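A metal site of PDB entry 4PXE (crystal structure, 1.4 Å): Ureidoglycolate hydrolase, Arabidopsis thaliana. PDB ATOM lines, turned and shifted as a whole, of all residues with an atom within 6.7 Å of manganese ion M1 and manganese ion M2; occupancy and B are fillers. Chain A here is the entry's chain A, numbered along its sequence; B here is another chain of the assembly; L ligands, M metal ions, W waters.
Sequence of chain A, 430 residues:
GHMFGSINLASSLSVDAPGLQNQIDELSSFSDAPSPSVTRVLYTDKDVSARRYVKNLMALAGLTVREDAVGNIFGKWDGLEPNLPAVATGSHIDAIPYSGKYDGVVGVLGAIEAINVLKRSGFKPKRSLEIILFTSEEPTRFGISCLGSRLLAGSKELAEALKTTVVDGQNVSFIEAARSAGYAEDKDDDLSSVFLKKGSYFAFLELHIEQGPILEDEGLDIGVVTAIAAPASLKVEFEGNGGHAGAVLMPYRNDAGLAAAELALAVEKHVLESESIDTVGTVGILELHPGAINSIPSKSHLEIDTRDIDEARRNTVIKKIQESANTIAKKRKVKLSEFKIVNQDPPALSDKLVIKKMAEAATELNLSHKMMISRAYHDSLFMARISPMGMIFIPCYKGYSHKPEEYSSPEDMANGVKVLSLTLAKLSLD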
ATOM      1  N   SER A  91      21.030  -1.644  22.118  1.00  0.00           N
ATOM      2  CA  SER A  91      21.021  -2.269  20.804  1.00  0.00           C
ATOM      3  C   SER A  91      20.047  -3.448  20.836  1.00  0.00           C
ATOM      4  O   SER A  91      19.199  -3.540  21.720  1.00  0.00           O
ATOM      5  CB  SER A  91      22.439  -2.706  20.413  1.00  0.00           C
ATOM      6  OG  SER A  91      22.584  -2.900  19.011  1.00  0.00           O
ATOM      7  N   HIS A  92      20.195  -4.352  19.867  1.00  0.00           N
ATOM      8  CA  HIS A  92      19.252  -5.473  19.732  1.00  0.00           C
ATOM      9  C   HIS A  92      19.974  -6.811  19.889  1.00  0.00           C
ATOM     10  O   HIS A  92      21.204  -6.877  19.772  1.00  0.00           O
ATOM     11  CB  HIS A  92      18.602  -5.431  18.343  1.00  0.00           C
ATOM     12  CG  HIS A  92      19.587  -5.605  17.228  1.00  0.00           C
ATOM     13  ND1 HIS A  92      19.765  -6.797  16.571  1.00  0.00           N
ATOM     14  CD2 HIS A  92      20.473  -4.729  16.682  1.00  0.00           C
ATOM     15  CE1 HIS A  92      20.718  -6.658  15.665  1.00  0.00           C
ATOM     16  NE2 HIS A  92      21.156  -5.414  15.709  1.00  0.00           N
ATOM     17  N   ASP A  94      18.138  -9.718  18.437  1.00  0.00           N
ATOM     18  CA  ASP A  94      17.614 -10.595  17.399  1.00  0.00           C
ATOM     19  C   ASP A  94      18.643 -10.754  16.262  1.00  0.00           C
ATOM     20  O   ASP A  94      19.509  -9.885  16.080  1.00  0.00           O
ATOM     21  CB  ASP A  94      16.178 -10.247  16.926  1.00  0.00           C
ATOM     22  CG  ASP A  94      16.036  -8.832  16.357  1.00  0.00           C
ATOM     23  OD1 ASP A  94      16.793  -7.904  16.714  1.00  0.00           O
ATOM     24  OD2 ASP A  94      15.071  -8.640  15.577  1.00  0.00           O
ATOM     25  N   ILE A  96      19.007 -12.299  12.137  1.00  0.00           N
ATOM     26  CA  ILE A  96      18.356 -12.837  10.938  1.00  0.00           C
ATOM     27  C   ILE A  96      18.836 -14.267  10.645  1.00  0.00           C
ATOM     28  O   ILE A  96      19.841 -14.714  11.189  1.00  0.00           O
ATOM     29  CB  ILE A  96      18.545 -11.915   9.696  1.00  0.00           C
ATOM     30  CG1 ILE A  96      19.969 -11.998   9.136  1.00  0.00           C
ATOM     31  CG2 ILE A  96      18.167 -10.481  10.032  1.00  0.00           C
ATOM     32  CD1 ILE A  96      20.147 -11.164   7.880  1.00  0.00           C
ATOM     33  N   TYR A 102      27.677 -11.168  16.584  1.00  0.00           N
ATOM     34  CA  TYR A 102      28.151  -9.860  17.052  1.00  0.00           C
ATOM     35  C   TYR A 102      27.214  -8.694  16.735  1.00  0.00           C
ATOM     36  O   TYR A 102      27.128  -7.722  17.498  1.00  0.00           O
ATOM     37  CB  TYR A 102      29.572  -9.580  16.504  1.00  0.00           C
ATOM     38  CG  TYR A 102      30.594 -10.590  16.954  1.00  0.00           C
ATOM     39  CD1 TYR A 102      31.344 -10.385  18.109  1.00  0.00           C
ATOM     40  CD2 TYR A 102      30.813 -11.757  16.220  1.00  0.00           C
ATOM     41  CE1 TYR A 102      32.271 -11.319  18.535  1.00  0.00           C
ATOM     42  CE2 TYR A 102      31.730 -12.690  16.637  1.00  0.00           C
ATOM     43  CZ  TYR A 102      32.464 -12.471  17.799  1.00  0.00           C
ATOM     44  OH  TYR A 102      33.381 -13.405  18.216  1.00  0.00           O
ATOM     45  N   ASP A 103      26.500  -8.804  15.620  1.00  0.00           N
ATOM     46  CA  ASP A 103      25.534  -7.790  15.213  1.00  0.00           C
ATOM     47  C   ASP A 103      24.502  -7.577  16.328  1.00  0.00           C
ATOM     48  O   ASP A 103      23.870  -8.523  16.777  1.00  0.00           O
ATOM     49  CB  ASP A 103      24.872  -8.255  13.922  1.00  0.00           C
ATOM     50  CG  ASP A 103      23.829  -7.313  13.424  1.00  0.00           C
ATOM     51  OD1 ASP A 103      23.838  -6.127  13.803  1.00  0.00           O
ATOM     52  OD2 ASP A 103      22.990  -7.746  12.623  1.00  0.00           O
ATOM     53  N   GLY A 104      24.382  -6.343  16.796  1.00  0.00           N
ATOM     54  CA  GLY A 104      23.468  -6.016  17.892  1.00  0.00           C
ATOM     55  C   GLY A 104      23.961  -6.420  19.276  1.00  0.00           C
ATOM     56  O   GLY A 104      23.991  -5.610  20.222  1.00  0.00           O
ATOM     57  N   VAL A 105      24.360  -7.689  19.389  1.00  0.00           N
ATOM     58  CA  VAL A 105      24.730  -8.253  20.678  1.00  0.00           C
ATOM     59  C   VAL A 105      25.864  -7.470  21.357  1.00  0.00           C
ATOM     60  O   VAL A 105      25.815  -7.247  22.568  1.00  0.00           O
ATOM     61  CB  VAL A 105      25.108  -9.745  20.550  1.00  0.00           C
ATOM     62  CG1 VAL A 105      25.533 -10.305  21.883  1.00  0.00           C
ATOM     63  CG2 VAL A 105      23.920 -10.546  20.019  1.00  0.00           C
ATOM     64  N   GLU A 137      15.096  -5.500  16.193  1.00  0.00           N
ATOM     65  CA  GLU A 137      15.539  -4.511  15.218  1.00  0.00           C
ATOM     66  C   GLU A 137      15.468  -5.075  13.795  1.00  0.00           C
ATOM     67  O   GLU A 137      15.357  -4.321  12.827  1.00  0.00           O
ATOM     68  CB  GLU A 137      16.964  -4.040  15.545  1.00  0.00           C
ATOM     69  CG  GLU A 137      17.487  -2.933  14.655  1.00  0.00           C
ATOM     70  CD  GLU A 137      18.261  -3.432  13.452  1.00  0.00           C
ATOM     71  OE1 GLU A 137      18.565  -4.652  13.364  1.00  0.00           O
ATOM     72  OE2 GLU A 137      18.564  -2.588  12.583  1.00  0.00           O
ATOM     73  N   GLU A 138      15.562  -6.397  13.671  1.00  0.00           N
ATOM     74  CA  GLU A 138      15.573  -7.030  12.344  1.00  0.00           C
ATOM     75  C   GLU A 138      14.159  -7.229  11.803  1.00  0.00           C
ATOM     76  O   GLU A 138      13.231  -7.467  12.570  1.00  0.00           O
ATOM     77  CB  GLU A 138      16.339  -8.343  12.388  1.00  0.00           C
ATOM     78  CG  GLU A 138      17.783  -8.184  12.849  1.00  0.00           C
ATOM     79  CD  GLU A 138      18.703  -7.679  11.777  1.00  0.00           C
ATOM     80  OE1 GLU A 138      18.262  -7.176  10.730  1.00  0.00           O
ATOM     81  OE2 GLU A 138      19.925  -7.821  12.017  1.00  0.00           O
ATOM     82  N   GLU A 206      24.778   4.202  20.688  1.00  0.00           N
ATOM     83  CA  GLU A 206      24.790   2.780  20.345  1.00  0.00           C
ATOM     84  C   GLU A 206      26.188   2.325  19.935  1.00  0.00           C
ATOM     85  O   GLU A 206      26.782   2.877  19.017  1.00  0.00           O
ATOM     86  CB  GLU A 206      23.808   2.504  19.213  1.00  0.00           C
ATOM     87  CG  GLU A 206      23.696   1.015  18.837  1.00  0.00           C
ATOM     88  CD  GLU A 206      22.498   0.685  17.956  1.00  0.00           C
ATOM     89  OE1 GLU A 206      21.811   1.614  17.456  1.00  0.00           O
ATOM     90  OE2 GLU A 206      22.241  -0.517  17.763  1.00  0.00           O
ATOM     91  N   HIS A 208      28.344  -0.570  18.174  1.00  0.00           N
ATOM     92  CA  HIS A 208      27.991  -1.553  17.146  1.00  0.00           C
ATOM     93  C   HIS A 208      29.219  -1.915  16.306  1.00  0.00           C
ATOM     94  O   HIS A 208      30.088  -1.071  16.078  1.00  0.00           O
ATOM     95  CB  HIS A 208      26.865  -1.018  16.237  1.00  0.00           C
ATOM     96  CG  HIS A 208      26.051  -2.077  15.552  1.00  0.00           C
ATOM     97  ND1 HIS A 208      26.537  -2.842  14.512  1.00  0.00           N
ATOM     98  CD2 HIS A 208      24.783  -2.516  15.784  1.00  0.00           C
ATOM     99  CE1 HIS A 208      25.601  -3.704  14.123  1.00  0.00           C
ATOM    100  NE2 HIS A 208      24.534  -3.520  14.876  1.00  0.00           N
ATOM    101  N   ILE A 209      29.296  -3.163  15.858  1.00  0.00           N
ATOM    102  CA  ILE A 209      30.338  -3.490  14.874  1.00  0.00           C
ATOM    103  C   ILE A 209      30.127  -2.664  13.606  1.00  0.00           C
ATOM    104  O   ILE A 209      28.996  -2.347  13.230  1.00  0.00           O
ATOM    105  CB  ILE A 209      30.393  -4.997  14.562  1.00  0.00           C
ATOM    106  CG1 ILE A 209      29.075  -5.477  13.933  1.00  0.00           C
ATOM    107  CG2 ILE A 209      30.714  -5.787  15.814  1.00  0.00           C
ATOM    108  CD1 ILE A 209      29.165  -6.897  13.299  1.00  0.00           C
ATOM    109  N   GLN A 211      30.325  -3.361  10.454  1.00  0.00           N
ATOM    110  CA  GLN A 211      29.690  -4.013   9.300  1.00  0.00           C
ATOM    111  C   GLN A 211      30.266  -3.485   7.989  1.00  0.00           C
ATOM    112  O   GLN A 211      29.578  -3.425   6.964  1.00  0.00           O
ATOM    113  CB  GLN A 211      28.165  -3.890   9.361  1.00  0.00           C
ATOM    114  CG  GLN A 211      27.613  -4.393  10.687  1.00  0.00           C
ATOM    115  CD  GLN A 211      26.109  -4.289  10.792  1.00  0.00           C
ATOM    116  OE1 GLN A 211      25.563  -3.198  10.930  1.00  0.00           O
ATOM    117  NE2 GLN A 211      25.436  -5.437  10.784  1.00  0.00           N
ATOM    118  N   ALA A 376      24.461   0.345   7.149  1.00  0.00           N
ATOM    119  CA  ALA A 376      23.387  -0.356   7.828  1.00  0.00           C
ATOM    120  C   ALA A 376      22.478   0.637   8.529  1.00  0.00           C
ATOM    121  O   ALA A 376      22.907   1.755   8.865  1.00  0.00           O
ATOM    122  CB  ALA A 376      23.963  -1.339   8.832  1.00  0.00           C
ATOM    123  N   TYR A 377      21.232   0.259   8.765  1.00  0.00           N
ATOM    124  CA  TYR A 377      20.407   1.034   9.694  1.00  0.00           C
ATOM    125  C   TYR A 377      20.495   0.401  11.078  1.00  0.00           C
ATOM    126  O   TYR A 377      21.047  -0.699  11.249  1.00  0.00           O
ATOM    127  CB  TYR A 377      18.945   1.181   9.199  1.00  0.00           C
ATOM    128  CG  TYR A 377      18.244  -0.126   8.900  1.00  0.00           C
ATOM    129  CD1 TYR A 377      18.112  -0.599   7.581  1.00  0.00           C
ATOM    130  CD2 TYR A 377      17.726  -0.908   9.920  1.00  0.00           C
ATOM    131  CE1 TYR A 377      17.481  -1.811   7.312  1.00  0.00           C
ATOM    132  CE2 TYR A 377      17.099  -2.110   9.668  1.00  0.00           C
ATOM    133  CZ  TYR A 377      16.965  -2.561   8.373  1.00  0.00           C
ATOM    134  OH  TYR A 377      16.345  -3.770   8.135  1.00  0.00           O
ATOM    135  N   HIS A 378      19.991   1.128  12.075  1.00  0.00           N
ATOM    136  CA  HIS A 378      20.102   0.731  13.471  1.00  0.00           C
ATOM    137  C   HIS A 378      18.963   1.361  14.236  1.00  0.00           C
ATOM    138  O   HIS A 378      18.336   2.297  13.752  1.00  0.00           O
ATOM    139  CB  HIS A 378      21.403   1.283  14.072  1.00  0.00           C
ATOM    140  CG  HIS A 378      22.650   0.845  13.361  1.00  0.00           C
ATOM    141  ND1 HIS A 378      23.235  -0.379  13.578  1.00  0.00           N
ATOM    142  CD2 HIS A 378      23.426   1.486  12.460  1.00  0.00           C
ATOM    143  CE1 HIS A 378      24.329  -0.467  12.842  1.00  0.00           C
ATOM    144  NE2 HIS A 378      24.466   0.645  12.150  1.00  0.00           N
ATOM    145  N   ASP A 379      18.734   0.899  15.461  1.00  0.00           N
ATOM    146  CA  ASP A 379      17.797   1.585  16.355  1.00  0.00           C
ATOM    147  C   ASP A 379      18.130   3.061  16.559  1.00  0.00           C
ATOM    148  O   ASP A 379      17.231   3.875  16.763  1.00  0.00           O
ATOM    149  CB  ASP A 379      17.732   0.847  17.690  1.00  0.00           C
ATOM    150  CG  ASP A 379      17.095  -0.533  17.542  1.00  0.00           C
ATOM    151  OD1 ASP A 379      15.918  -0.565  17.135  1.00  0.00           O
ATOM    152  OD2 ASP A 379      17.761  -1.556  17.804  1.00  0.00           O
ATOM    153  N   SER A 401      29.224  -9.280   7.746  1.00  0.00           N
ATOM    154  CA  SER A 401      28.091  -9.264   8.662  1.00  0.00           C
ATOM    155  C   SER A 401      26.905  -9.970   8.007  1.00  0.00           C
ATOM    156  O   SER A 401      26.892 -10.201   6.794  1.00  0.00           O
ATOM    157  CB  SER A 401      27.752  -7.828   9.083  1.00  0.00           C
ATOM    158  OG  SER A 401      26.888  -7.813  10.195  1.00  0.00           O
ATOM    159  N   HIS A 402      25.918 -10.338   8.813  1.00  0.00           N
ATOM    160  CA  HIS A 402      24.756 -11.120   8.361  1.00  0.00           C
ATOM    161  C   HIS A 402      25.167 -12.463   7.775  1.00  0.00           C
ATOM    162  O   HIS A 402      24.531 -12.996   6.874  1.00  0.00           O
ATOM    163  CB  HIS A 402      23.910 -10.324   7.367  1.00  0.00           C
ATOM    164  CG  HIS A 402      23.031  -9.303   8.018  1.00  0.00           C
ATOM    165  ND1 HIS A 402      22.157  -8.501   7.309  1.00  0.00           N
ATOM    166  CD2 HIS A 402      22.895  -8.956   9.319  1.00  0.00           C
ATOM    167  CE1 HIS A 402      21.516  -7.712   8.143  1.00  0.00           C
ATOM    168  NE2 HIS A 402      21.940  -7.967   9.364  1.00  0.00           N
ATOM    169  N   GLU A 406      31.140 -13.324  10.387  1.00  0.00           N
ATOM    170  CA  GLU A 406      31.182 -12.104  11.187  1.00  0.00           C
ATOM    171  C   GLU A 406      32.070 -12.293  12.424  1.00  0.00           C
ATOM    172  O   GLU A 406      31.942 -13.277  13.141  1.00  0.00           O
ATOM    173  CB  GLU A 406      29.760 -11.736  11.611  1.00  0.00           C
ATOM    174  CG  GLU A 406      29.605 -10.442  12.392  1.00  0.00           C
ATOM    175  CD  GLU A 406      28.159 -10.235  12.756  1.00  0.00           C
ATOM    176  OE1 GLU A 406      27.768 -10.700  13.843  1.00  0.00           O
ATOM    177  OE2 GLU A 406      27.405  -9.672  11.925  1.00  0.00           O
ATOM    178  N   HIS B 244      25.856  -8.544   4.028  1.00  0.00           N
ATOM    179  CA  HIS B 244      24.913  -7.526   4.454  1.00  0.00           C
ATOM    180  C   HIS B 244      24.385  -6.710   3.277  1.00  0.00           C
ATOM    181  O   HIS B 244      25.140  -6.063   2.561  1.00  0.00           O
ATOM    182  CB  HIS B 244      25.621  -6.605   5.452  1.00  0.00           C
ATOM    183  CG  HIS B 244      24.682  -5.825   6.286  1.00  0.00           C
ATOM    184  ND1 HIS B 244      23.893  -4.810   5.782  1.00  0.00           N
ATOM    185  CD2 HIS B 244      24.396  -5.885   7.620  1.00  0.00           C
ATOM    186  CE1 HIS B 244      23.170  -4.289   6.750  1.00  0.00           C
ATOM    187  NE2 HIS B 244      23.445  -4.925   7.879  1.00  0.00           N
ATOM    188  N   ASN B 294      17.328  -8.606   4.061  1.00  0.00           N
ATOM    189  CA  ASN B 294      18.544  -7.824   4.219  1.00  0.00           C
ATOM    190  C   ASN B 294      19.829  -8.672   4.238  1.00  0.00           C
ATOM    191  O   ASN B 294      20.878  -8.261   4.778  1.00  0.00           O
ATOM    192  CB  ASN B 294      18.436  -6.895   5.442  1.00  0.00           C
ATOM    193  CG  ASN B 294      18.043  -7.617   6.732  1.00  0.00           C
ATOM    194  OD1 ASN B 294      17.567  -8.759   6.717  1.00  0.00           O
ATOM    195  ND2 ASN B 294      18.231  -6.934   7.863  1.00  0.00           N
HETATM  196  C1  LIG L   1      19.758  -4.183   9.791  1.00  0.00           C
HETATM  197  O1  LIG L   1      20.154  -3.296  10.784  1.00  0.00           O
HETATM  198  C2  LIG L   1      20.147  -3.781   8.415  1.00  0.00           C
HETATM  199  O2  LIG L   1      20.805  -2.704   8.253  1.00  0.00           O
HETATM  200  O3  LIG L   1      19.824  -4.506   7.433  1.00  0.00           O
HETATM  201 MN    MN M   1      21.606  -6.688  11.264  1.00  0.00          MN
HETATM  202 MN    MN M   2      22.518  -4.415  14.152  1.00  0.00          MN
HETATM  203  O   HOH W   1      21.605  -2.419  14.537  1.00  0.00           O
HETATM  204  O   HOH W   2      22.653  -5.436  10.444  1.00  0.00           O
HETATM  205  O   HOH W   3      21.032  -5.198  12.689  1.00  0.00           O
HETATM  206  O   HOH W   4      23.017  -3.217  12.039  1.00  0.00           O
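The side-chain carboxylate of Glu 137 lies close to an oxygen (O1) of the ligand, 2.5 Å away. O2 of the ligand is in hydrogen-bond range of N of Tyr 377 (3.0 Å). The side-chain amide nitrogen of Asn 294 of chain B lies within hydrogen-bond range of an oxygen (O3) of the ligand (2.9 Å). A ring nitrogen (NE2) of His 244 of chain B lies close to an oxygen (O2) of the ligand, at 3.5 Å.
O of Gly 104 sits at hydrogen-bond distance from OG of Ser 91 (3.3 Å). OE1 of Glu 138 is in hydrogen-bond range of ND2 of Asn 294 of chain B, 2.9 Å away. N of Glu 138 is in hydrogen-bond range of OD2 of Asp 94 (3.0 Å). The backbone carbonyl oxygen (O) of His 92 is in hydrogen-bond range of the backbone NH (N) of Val 105. A ring nitrogen (ND1) of His 92 lies within hydrogen-bond range of the backbone carbonyl oxygen (O) of Asp 94, at 3.1 Å. A ring nitrogen (ND1) of His 402 is in hydrogen-bond range of the backbone carbonyl oxygen (O) of Asn 294 of chain B, 2.8 Å away. OD1 of Asp 103 sits close to NE2 of Gln 211, 3.5 Å away. N of Asp 103 lies within hydrogen-bond range of OE1 of Glu 406 (2.9 Å).
Merely in contact with manganese ion M2: Gly 104 (3.8 Å). Of the 23 residues printed, 4 come within 4 Å of manganese ion M2.
Manganese ion M1 is bound by water W2 (1.8 Å), water W3 (2.1 Å), OE2 of Glu 138 (2.2 Å), OD2 of Asp 103 (2.2 Å) and NE2 of His 402 (2.3 Å).
Manganese ion M2 is bound by the side-chain carboxylate of Asp 103 (2.2 Å), water W3 (2.2 Å), water W1 (2.2 Å), a ring nitrogen (NE2) of His 92 (2.3 Å), a ring nitrogen (NE2) of His 208 (2.3 Å) and water W4 (2.5 Å). Manganese ion M2 has six donor atoms within binding distance.
Water W3 lies within hydrogen-bond range of the side-chain carboxylate of Glu 137 (2.6 Å) and an oxygen (O1) of the ligand (2.8 Å). Water W2 lies within hydrogen-bond range of a ring nitrogen (NE2) of His 244 of chain B (2.7 Å), the side-chain amide nitrogen (NE2) of Gln 211 (2.8 Å) and an oxygen (O1) of the ligand (3.3 Å).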
